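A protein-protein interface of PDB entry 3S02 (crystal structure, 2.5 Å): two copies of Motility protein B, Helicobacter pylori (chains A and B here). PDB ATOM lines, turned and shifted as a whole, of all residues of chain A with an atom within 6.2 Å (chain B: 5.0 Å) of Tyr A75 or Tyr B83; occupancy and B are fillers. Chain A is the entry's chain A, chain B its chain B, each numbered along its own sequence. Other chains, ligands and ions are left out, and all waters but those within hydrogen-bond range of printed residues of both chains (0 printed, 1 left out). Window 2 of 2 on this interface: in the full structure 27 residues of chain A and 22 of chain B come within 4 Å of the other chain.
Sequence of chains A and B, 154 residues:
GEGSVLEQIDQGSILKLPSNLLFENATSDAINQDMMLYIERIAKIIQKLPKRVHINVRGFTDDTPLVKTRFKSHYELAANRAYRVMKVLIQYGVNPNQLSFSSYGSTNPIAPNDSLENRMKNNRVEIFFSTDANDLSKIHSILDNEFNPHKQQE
The backbone carbonyl oxygen (O) of Phe B101 sits at hydrogen-bond distance from the backbone NH (N) of Ser A103.
The backbone carbonyl oxygen of Tyr A75 sits at hydrogen-bond distance from the side-chain hydroxyl of Ser A103. The backbone NH (N) of Gly A105 is in hydrogen-bond range of the side-chain hydroxyl (OG) of Ser A103, 3.4 Å away. OG1 of Thr A107 is in hydrogen-bond range of O of Tyr A104, 2.6 Å away.
Tyr A75 touches Tyr B83 (CD2 to CE1, 3.4 Å). Tyr A75 touches Met B86 (CZ to CE, 3.4 Å). Ile B90 touches Tyr A75 (CD1 to OH, 3.7 Å). Tyr A75 touches Phe B101 (CB to CE2, 3.9 Å). Thr A107 touches Pro B96 (CG2 to O, 3.6 Å).
Tyr A75 touches four residues of chain B. Of the printed residues of chain B, Ser A103 touches Phe B101 (3.0 Å). Of the printed residues of chain B, Thr A107 touches Pro B96 (3.6 Å). Of chain A, only Tyr A75 (3.4 Å) comes within 4 Å of Tyr B83. Printed residues of chain A within 4 Å of Met B86: Tyr A75 (3.4 Å). Of the printed residues of chain A, Ile B90 touches Tyr A75 (3.7 Å). The nearest printed residue of chain B that does not touch Ser A103 is Met B86 (5.2 Å).
Hydrophobic or aromatic side chains of chain B within 4 Å of the printed part of chain A: Tyr B83, Met B86, Ile B90 and Phe B101. Along chain B the printed residues that touch a printed residue of chain A span positions 83 to 101. Hydrophobic or aromatic side chains of chain A that line the printed part of chain B: Tyr A75. Among the printed residues, 6 pairs touch across the chains.
3 positions are printed for both chains. Of the 6 pairs that touch across the chains among the printed residues, none has its exchanged pair printed and touching as well.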
ATOM      1  N   THR A  61      17.314  -7.648  -1.614  1.00  0.00           N
ATOM      2  CA  THR A  61      16.893  -7.228  -0.305  1.00  0.00           C
ATOM      3  C   THR A  61      15.820  -6.145  -0.472  1.00  0.00           C
ATOM      4  O   THR A  61      15.723  -5.531  -1.551  1.00  0.00           O
ATOM      5  CB  THR A  61      18.071  -6.632   0.486  1.00  0.00           C
ATOM      6  OG1 THR A  61      18.544  -5.469  -0.199  1.00  0.00           O
ATOM      7  CG2 THR A  61      19.195  -7.630   0.641  1.00  0.00           C
ATOM      8  N   SER A  73      26.277  -2.038   2.912  1.00  0.00           N
ATOM      9  CA  SER A  73      25.171  -1.728   1.983  1.00  0.00           C
ATOM     10  C   SER A  73      24.362  -2.963   1.690  1.00  0.00           C
ATOM     11  O   SER A  73      24.794  -4.074   1.945  1.00  0.00           O
ATOM     12  CB  SER A  73      25.678  -1.145   0.660  1.00  0.00           C
ATOM     13  OG  SER A  73      26.586  -2.037   0.018  1.00  0.00           O
ATOM     14  N   HIS A  74      23.178  -2.742   1.147  1.00  0.00           N
ATOM     15  CA  HIS A  74      22.357  -3.801   0.596  1.00  0.00           C
ATOM     16  C   HIS A  74      23.083  -4.629  -0.474  1.00  0.00           C
ATOM     17  O   HIS A  74      23.068  -5.857  -0.402  1.00  0.00           O
ATOM     18  CB  HIS A  74      21.021  -3.228   0.117  1.00  0.00           C
ATOM     19  CG  HIS A  74      20.181  -2.707   1.241  1.00  0.00           C
ATOM     20  ND1 HIS A  74      19.899  -1.365   1.407  1.00  0.00           N
ATOM     21  CD2 HIS A  74      19.592  -3.348   2.285  1.00  0.00           C
ATOM     22  CE1 HIS A  74      19.149  -1.209   2.486  1.00  0.00           C
ATOM     23  NE2 HIS A  74      18.950  -2.395   3.036  1.00  0.00           N
ATOM     24  N   TYR A  75      23.777  -3.976  -1.402  1.00  0.00           N
ATOM     25  CA  TYR A  75      24.592  -4.704  -2.384  1.00  0.00           C
ATOM     26  C   TYR A  75      25.416  -5.778  -1.725  1.00  0.00           C
ATOM     27  O   TYR A  75      25.447  -6.927  -2.193  1.00  0.00           O
ATOM     28  CB  TYR A  75      25.536  -3.793  -3.168  1.00  0.00           C
ATOM     29  CG  TYR A  75      24.843  -2.947  -4.204  1.00  0.00           C
ATOM     30  CD1 TYR A  75      23.943  -3.518  -5.114  1.00  0.00           C
ATOM     31  CD2 TYR A  75      25.100  -1.574  -4.295  1.00  0.00           C
ATOM     32  CE1 TYR A  75      23.311  -2.752  -6.067  1.00  0.00           C
ATOM     33  CE2 TYR A  75      24.452  -0.785  -5.255  1.00  0.00           C
ATOM     34  CZ  TYR A  75      23.565  -1.387  -6.130  1.00  0.00           C
ATOM     35  OH  TYR A  75      22.926  -0.622  -7.079  1.00  0.00           O
ATOM     36  N   GLU A  76      26.067  -5.385  -0.635  1.00  0.00           N
ATOM     37  CA  GLU A  76      26.991  -6.253   0.060  1.00  0.00           C
ATOM     38  C   GLU A  76      26.233  -7.374   0.785  1.00  0.00           C
ATOM     39  O   GLU A  76      26.633  -8.538   0.729  1.00  0.00           O
ATOM     40  CB  GLU A  76      27.852  -5.447   1.037  1.00  0.00           C
ATOM     41  CG  GLU A  76      28.968  -6.295   1.632  1.00  0.00           C
ATOM     42  CD  GLU A  76      29.870  -5.584   2.625  1.00  0.00           C
ATOM     43  OE1 GLU A  76      29.589  -4.428   2.980  1.00  0.00           O
ATOM     44  OE2 GLU A  76      30.870  -6.197   3.060  1.00  0.00           O
ATOM     45  N   LEU A  77      25.157  -7.016   1.480  1.00  0.00           N
ATOM     46  CA  LEU A  77      24.336  -8.005   2.185  1.00  0.00           C
ATOM     47  C   LEU A  77      23.802  -9.039   1.185  1.00  0.00           C
ATOM     48  O   LEU A  77      23.891 -10.247   1.431  1.00  0.00           O
ATOM     49  CB  LEU A  77      23.170  -7.334   2.939  1.00  0.00           C
ATOM     50  CG  LEU A  77      22.069  -8.260   3.470  1.00  0.00           C
ATOM     51  CD1 LEU A  77      22.631  -9.320   4.419  1.00  0.00           C
ATOM     52  CD2 LEU A  77      20.978  -7.427   4.157  1.00  0.00           C
ATOM     53  N   ALA A  78      23.280  -8.557   0.053  1.00  0.00           N
ATOM     54  CA  ALA A  78      22.768  -9.447  -0.973  1.00  0.00           C
ATOM     55  C   ALA A  78      23.908 -10.334  -1.553  1.00  0.00           C
ATOM     56  O   ALA A  78      23.702 -11.563  -1.760  1.00  0.00           O
ATOM     57  CB  ALA A  78      22.034  -8.646  -2.076  1.00  0.00           C
ATOM     58  N   ALA A  79      25.090  -9.742  -1.793  1.00  0.00           N
ATOM     59  CA  ALA A  79      26.226 -10.500  -2.334  1.00  0.00           C
ATOM     60  C   ALA A  79      26.641 -11.622  -1.392  1.00  0.00           C
ATOM     61  O   ALA A  79      26.822 -12.780  -1.836  1.00  0.00           O
ATOM     62  CB  ALA A  79      27.425  -9.599  -2.676  1.00  0.00           C
ATOM     63  N   ASN A  80      26.760 -11.301  -0.098  1.00  0.00           N
ATOM     64  CA  ASN A  80      27.170 -12.310   0.878  1.00  0.00           C
ATOM     65  C   ASN A  80      26.128 -13.416   1.011  1.00  0.00           C
ATOM     66  O   ASN A  80      26.462 -14.609   1.094  1.00  0.00           O
ATOM     67  CB  ASN A  80      27.526 -11.687   2.227  1.00  0.00           C
ATOM     68  CG  ASN A  80      28.939 -11.108   2.236  1.00  0.00           C
ATOM     69  OD1 ASN A  80      29.895 -11.820   2.511  1.00  0.00           O
ATOM     70  ND2 ASN A  80      29.075  -9.815   1.914  1.00  0.00           N
ATOM     71  N   SER A 103      24.354  -9.922  -7.071  1.00  0.00           N
ATOM     72  CA  SER A 103      23.684  -9.034  -6.111  1.00  0.00           C
ATOM     73  C   SER A 103      22.916  -7.924  -6.845  1.00  0.00           C
ATOM     74  O   SER A 103      23.448  -7.248  -7.747  1.00  0.00           O
ATOM     75  CB  SER A 103      24.710  -8.444  -5.125  1.00  0.00           C
ATOM     76  OG  SER A 103      24.137  -7.423  -4.330  1.00  0.00           O
ATOM     77  N   TYR A 104      21.649  -7.769  -6.476  1.00  0.00           N
ATOM     78  CA  TYR A 104      20.807  -6.693  -6.987  1.00  0.00           C
ATOM     79  C   TYR A 104      20.635  -5.623  -5.909  1.00  0.00           C
ATOM     80  O   TYR A 104      20.076  -4.556  -6.162  1.00  0.00           O
ATOM     81  CB  TYR A 104      19.459  -7.259  -7.442  1.00  0.00           C
ATOM     82  CG  TYR A 104      19.609  -8.144  -8.655  1.00  0.00           C
ATOM     83  CD1 TYR A 104      19.266  -7.671  -9.936  1.00  0.00           C
ATOM     84  CD2 TYR A 104      20.164  -9.423  -8.542  1.00  0.00           C
ATOM     85  CE1 TYR A 104      19.445  -8.458 -11.058  1.00  0.00           C
ATOM     86  CE2 TYR A 104      20.353 -10.210  -9.652  1.00  0.00           C
ATOM     87  CZ  TYR A 104      19.996  -9.722 -10.912  1.00  0.00           C
ATOM     88  OH  TYR A 104      20.176 -10.521 -12.019  1.00  0.00           O
ATOM     89  N   GLY A 105      21.154  -5.897  -4.714  1.00  0.00           N
ATOM     90  CA  GLY A 105      20.909  -5.028  -3.565  1.00  0.00           C
ATOM     91  C   GLY A 105      19.412  -4.790  -3.383  1.00  0.00           C
ATOM     92  O   GLY A 105      18.616  -5.740  -3.354  1.00  0.00           O
ATOM     93  N   SER A 106      19.028  -3.517  -3.288  1.00  0.00           N
ATOM     94  CA  SER A 106      17.629  -3.174  -3.054  1.00  0.00           C
ATOM     95  C   SER A 106      16.945  -2.700  -4.313  1.00  0.00           C
ATOM     96  O   SER A 106      15.777  -2.322  -4.293  1.00  0.00           O
ATOM     97  CB  SER A 106      17.509  -2.122  -1.959  1.00  0.00           C
ATOM     98  OG  SER A 106      18.321  -0.992  -2.248  1.00  0.00           O
ATOM     99  N   THR A 107      17.688  -2.733  -5.409  1.00  0.00           N
ATOM    100  CA  THR A 107      17.201  -2.291  -6.701  1.00  0.00           C
ATOM    101  C   THR A 107      16.191  -3.236  -7.317  1.00  0.00           C
ATOM    102  O   THR A 107      16.193  -4.445  -7.056  1.00  0.00           O
ATOM    103  CB  THR A 107      18.318  -2.242  -7.716  1.00  0.00           C
ATOM    104  OG1 THR A 107      18.662  -3.599  -8.077  1.00  0.00           O
ATOM    105  CG2 THR A 107      19.529  -1.458  -7.152  1.00  0.00           C
ATOM    106  N   ALA B  78      36.769 -10.800  -7.432  1.00  0.00           N
ATOM    107  CA  ALA B  78      35.997 -10.632  -8.665  1.00  0.00           C
ATOM    108  C   ALA B  78      34.671  -9.909  -8.394  1.00  0.00           C
ATOM    109  O   ALA B  78      34.192  -9.110  -9.233  1.00  0.00           O
ATOM    110  CB  ALA B  78      35.737 -11.974  -9.323  1.00  0.00           C
ATOM    111  N   ALA B  79      34.083 -10.177  -7.227  1.00  0.00           N
ATOM    112  CA  ALA B  79      32.861  -9.478  -6.855  1.00  0.00           C
ATOM    113  C   ALA B  79      33.130  -7.974  -6.732  1.00  0.00           C
ATOM    114  O   ALA B  79      32.374  -7.151  -7.250  1.00  0.00           O
ATOM    115  CB  ALA B  79      32.286 -10.039  -5.556  1.00  0.00           C
ATOM    116  N   ASN B  80      34.208  -7.618  -6.041  1.00  0.00           N
ATOM    117  CA  ASN B  80      34.495  -6.205  -5.761  1.00  0.00           C
ATOM    118  C   ASN B  80      34.827  -5.446  -7.013  1.00  0.00           C
ATOM    119  O   ASN B  80      34.389  -4.312  -7.183  1.00  0.00           O
ATOM    120  CB  ASN B  80      35.577  -6.039  -4.683  1.00  0.00           C
ATOM    121  CG  ASN B  80      35.002  -6.181  -3.286  1.00  0.00           C
ATOM    122  OD1 ASN B  80      34.490  -5.218  -2.723  1.00  0.00           O
ATOM    123  ND2 ASN B  80      35.041  -7.399  -2.738  1.00  0.00           N
ATOM    124  N   ARG B  81      35.548  -6.099  -7.907  1.00  0.00           N
ATOM    125  CA  ARG B  81      35.866  -5.510  -9.186  1.00  0.00           C
ATOM    126  C   ARG B  81      34.614  -5.252 -10.028  1.00  0.00           C
ATOM    127  O   ARG B  81      34.451  -4.145 -10.578  1.00  0.00           O
ATOM    128  CB  ARG B  81      36.901  -6.360  -9.925  1.00  0.00           C
ATOM    129  CG  ARG B  81      38.307  -6.129  -9.363  1.00  0.00           C
ATOM    130  CD  ARG B  81      39.240  -7.261  -9.628  1.00  0.00           C
ATOM    131  NE  ARG B  81      39.733  -7.194 -10.989  1.00  0.00           N
ATOM    132  CZ  ARG B  81      40.959  -6.816 -11.345  1.00  0.00           C
ATOM    133  NH1 ARG B  81      41.867  -6.458 -10.440  1.00  0.00           N
ATOM    134  NH2 ARG B  81      41.270  -6.805 -12.630  1.00  0.00           N
ATOM    135  N   ALA B  82      33.722  -6.240 -10.090  1.00  0.00           N
ATOM    136  CA  ALA B  82      32.513  -6.105 -10.872  1.00  0.00           C
ATOM    137  C   ALA B  82      31.699  -4.996 -10.248  1.00  0.00           C
ATOM    138  O   ALA B  82      31.186  -4.114 -10.947  1.00  0.00           O
ATOM    139  CB  ALA B  82      31.747  -7.399 -10.899  1.00  0.00           C
ATOM    140  N   TYR B  83      31.620  -5.014  -8.924  1.00  0.00           N
ATOM    141  CA  TYR B  83      30.924  -3.963  -8.190  1.00  0.00           C
ATOM    142  C   TYR B  83      31.450  -2.551  -8.508  1.00  0.00           C
ATOM    143  O   TYR B  83      30.638  -1.656  -8.784  1.00  0.00           O
ATOM    144  CB  TYR B  83      30.961  -4.255  -6.678  1.00  0.00           C
ATOM    145  CG  TYR B  83      30.349  -3.173  -5.821  1.00  0.00           C
ATOM    146  CD1 TYR B  83      28.967  -2.974  -5.798  1.00  0.00           C
ATOM    147  CD2 TYR B  83      31.157  -2.316  -5.065  1.00  0.00           C
ATOM    148  CE1 TYR B  83      28.401  -1.959  -5.028  1.00  0.00           C
ATOM    149  CE2 TYR B  83      30.602  -1.294  -4.286  1.00  0.00           C
ATOM    150  CZ  TYR B  83      29.229  -1.137  -4.269  1.00  0.00           C
ATOM    151  OH  TYR B  83      28.672  -0.148  -3.514  1.00  0.00           O
ATOM    152  N   ARG B  84      32.777  -2.341  -8.478  1.00  0.00           N
ATOM    153  CA  ARG B  84      33.324  -1.003  -8.762  1.00  0.00           C
ATOM    154  C   ARG B  84      32.911  -0.507 -10.123  1.00  0.00           C
ATOM    155  O   ARG B  84      32.460   0.626 -10.230  1.00  0.00           O
ATOM    156  CB  ARG B  84      34.845  -0.915  -8.654  1.00  0.00           C
ATOM    157  CG  ARG B  84      35.377  -1.033  -7.226  1.00  0.00           C
ATOM    158  CD  ARG B  84      34.945   0.121  -6.320  1.00  0.00           C
ATOM    159  NE  ARG B  84      34.938  -0.295  -4.913  1.00  0.00           N
ATOM    160  CZ  ARG B  84      34.301   0.354  -3.931  1.00  0.00           C
ATOM    161  NH1 ARG B  84      33.596   1.464  -4.201  1.00  0.00           N
ATOM    162  NH2 ARG B  84      34.365  -0.107  -2.676  1.00  0.00           N
ATOM    163  N   VAL B  85      33.070  -1.338 -11.152  1.00  0.00           N
ATOM    164  CA  VAL B  85      32.576  -0.999 -12.476  1.00  0.00           C
ATOM    165  C   VAL B  85      31.079  -0.684 -12.453  1.00  0.00           C
ATOM    166  O   VAL B  85      30.658   0.357 -12.945  1.00  0.00           O
ATOM    167  CB  VAL B  85      32.932  -2.056 -13.570  1.00  0.00           C
ATOM    168  CG1 VAL B  85      32.321  -1.640 -14.931  1.00  0.00           C
ATOM    169  CG2 VAL B  85      34.446  -2.165 -13.720  1.00  0.00           C
ATOM    170  N   MET B  86      30.279  -1.548 -11.850  1.00  0.00           N
ATOM    171  CA  MET B  86      28.887  -1.220 -11.694  1.00  0.00           C
ATOM    172  C   MET B  86      28.696   0.193 -11.093  1.00  0.00           C
ATOM    173  O   MET B  86      27.858   0.981 -11.576  1.00  0.00           O
ATOM    174  CB  MET B  86      28.146  -2.285 -10.888  1.00  0.00           C
ATOM    175  CG  MET B  86      26.628  -2.092 -10.929  1.00  0.00           C
ATOM    176  SD  MET B  86      25.731  -3.024  -9.693  1.00  0.00           S
ATOM    177  CE  MET B  86      26.135  -2.116  -8.214  1.00  0.00           C
ATOM    178  N   LYS B  87      29.465   0.523 -10.056  1.00  0.00           N
ATOM    179  CA  LYS B  87      29.305   1.828  -9.378  1.00  0.00           C
ATOM    180  C   LYS B  87      29.698   3.014 -10.282  1.00  0.00           C
ATOM    181  O   LYS B  87      29.006   4.043 -10.314  1.00  0.00           O
ATOM    182  CB  LYS B  87      30.100   1.885  -8.071  1.00  0.00           C
ATOM    183  CG  LYS B  87      29.467   1.135  -6.920  1.00  0.00           C
ATOM    184  CD  LYS B  87      28.258   1.863  -6.300  1.00  0.00           C
ATOM    185  CE  LYS B  87      28.676   2.882  -5.229  1.00  0.00           C
ATOM    186  NZ  LYS B  87      27.536   3.777  -4.825  1.00  0.00           N
ATOM    187  N   ILE B  90      26.908   3.731 -12.603  1.00  0.00           N
ATOM    188  CA  ILE B  90      25.895   4.542 -11.947  1.00  0.00           C
ATOM    189  C   ILE B  90      26.369   6.028 -11.939  1.00  0.00           C
ATOM    190  O   ILE B  90      25.670   6.932 -12.396  1.00  0.00           O
ATOM    191  CB  ILE B  90      25.557   3.953 -10.535  1.00  0.00           C
ATOM    192  CG1 ILE B  90      24.941   2.541 -10.695  1.00  0.00           C
ATOM    193  CG2 ILE B  90      24.685   4.904  -9.704  1.00  0.00           C
ATOM    194  CD1 ILE B  90      24.592   1.802  -9.373  1.00  0.00           C
ATOM    195  N   PRO B  96      20.377   2.670 -11.739  1.00  0.00           N
ATOM    196  CA  PRO B  96      20.665   1.584 -10.777  1.00  0.00           C
ATOM    197  C   PRO B  96      19.720   0.404 -10.905  1.00  0.00           C
ATOM    198  O   PRO B  96      20.126  -0.727 -10.664  1.00  0.00           O
ATOM    199  CB  PRO B  96      20.453   2.244  -9.403  1.00  0.00           C
ATOM    200  CG  PRO B  96      20.586   3.701  -9.630  1.00  0.00           C
ATOM    201  CD  PRO B  96      20.318   3.995 -11.091  1.00  0.00           C
ATOM    202  N   PHE B 101      25.665  -7.009 -10.200  1.00  0.00           N
ATOM    203  CA  PHE B 101      27.033  -7.513 -10.366  1.00  0.00           C
ATOM    204  C   PHE B 101      27.165  -8.968  -9.978  1.00  0.00           C
ATOM    205  O   PHE B 101      26.422  -9.450  -9.133  1.00  0.00           O
ATOM    206  CB  PHE B 101      28.090  -6.633  -9.665  1.00  0.00           C
ATOM    207  CG  PHE B 101      28.026  -6.648  -8.169  1.00  0.00           C
ATOM    208  CD1 PHE B 101      28.843  -7.505  -7.441  1.00  0.00           C
ATOM    209  CD2 PHE B 101      27.207  -5.767  -7.482  1.00  0.00           C
ATOM    210  CE1 PHE B 101      28.823  -7.527  -6.045  1.00  0.00           C
ATOM    211  CE2 PHE B 101      27.169  -5.762  -6.062  1.00  0.00           C
ATOM    212  CZ  PHE B 101      27.968  -6.654  -5.352  1.00  0.00           C
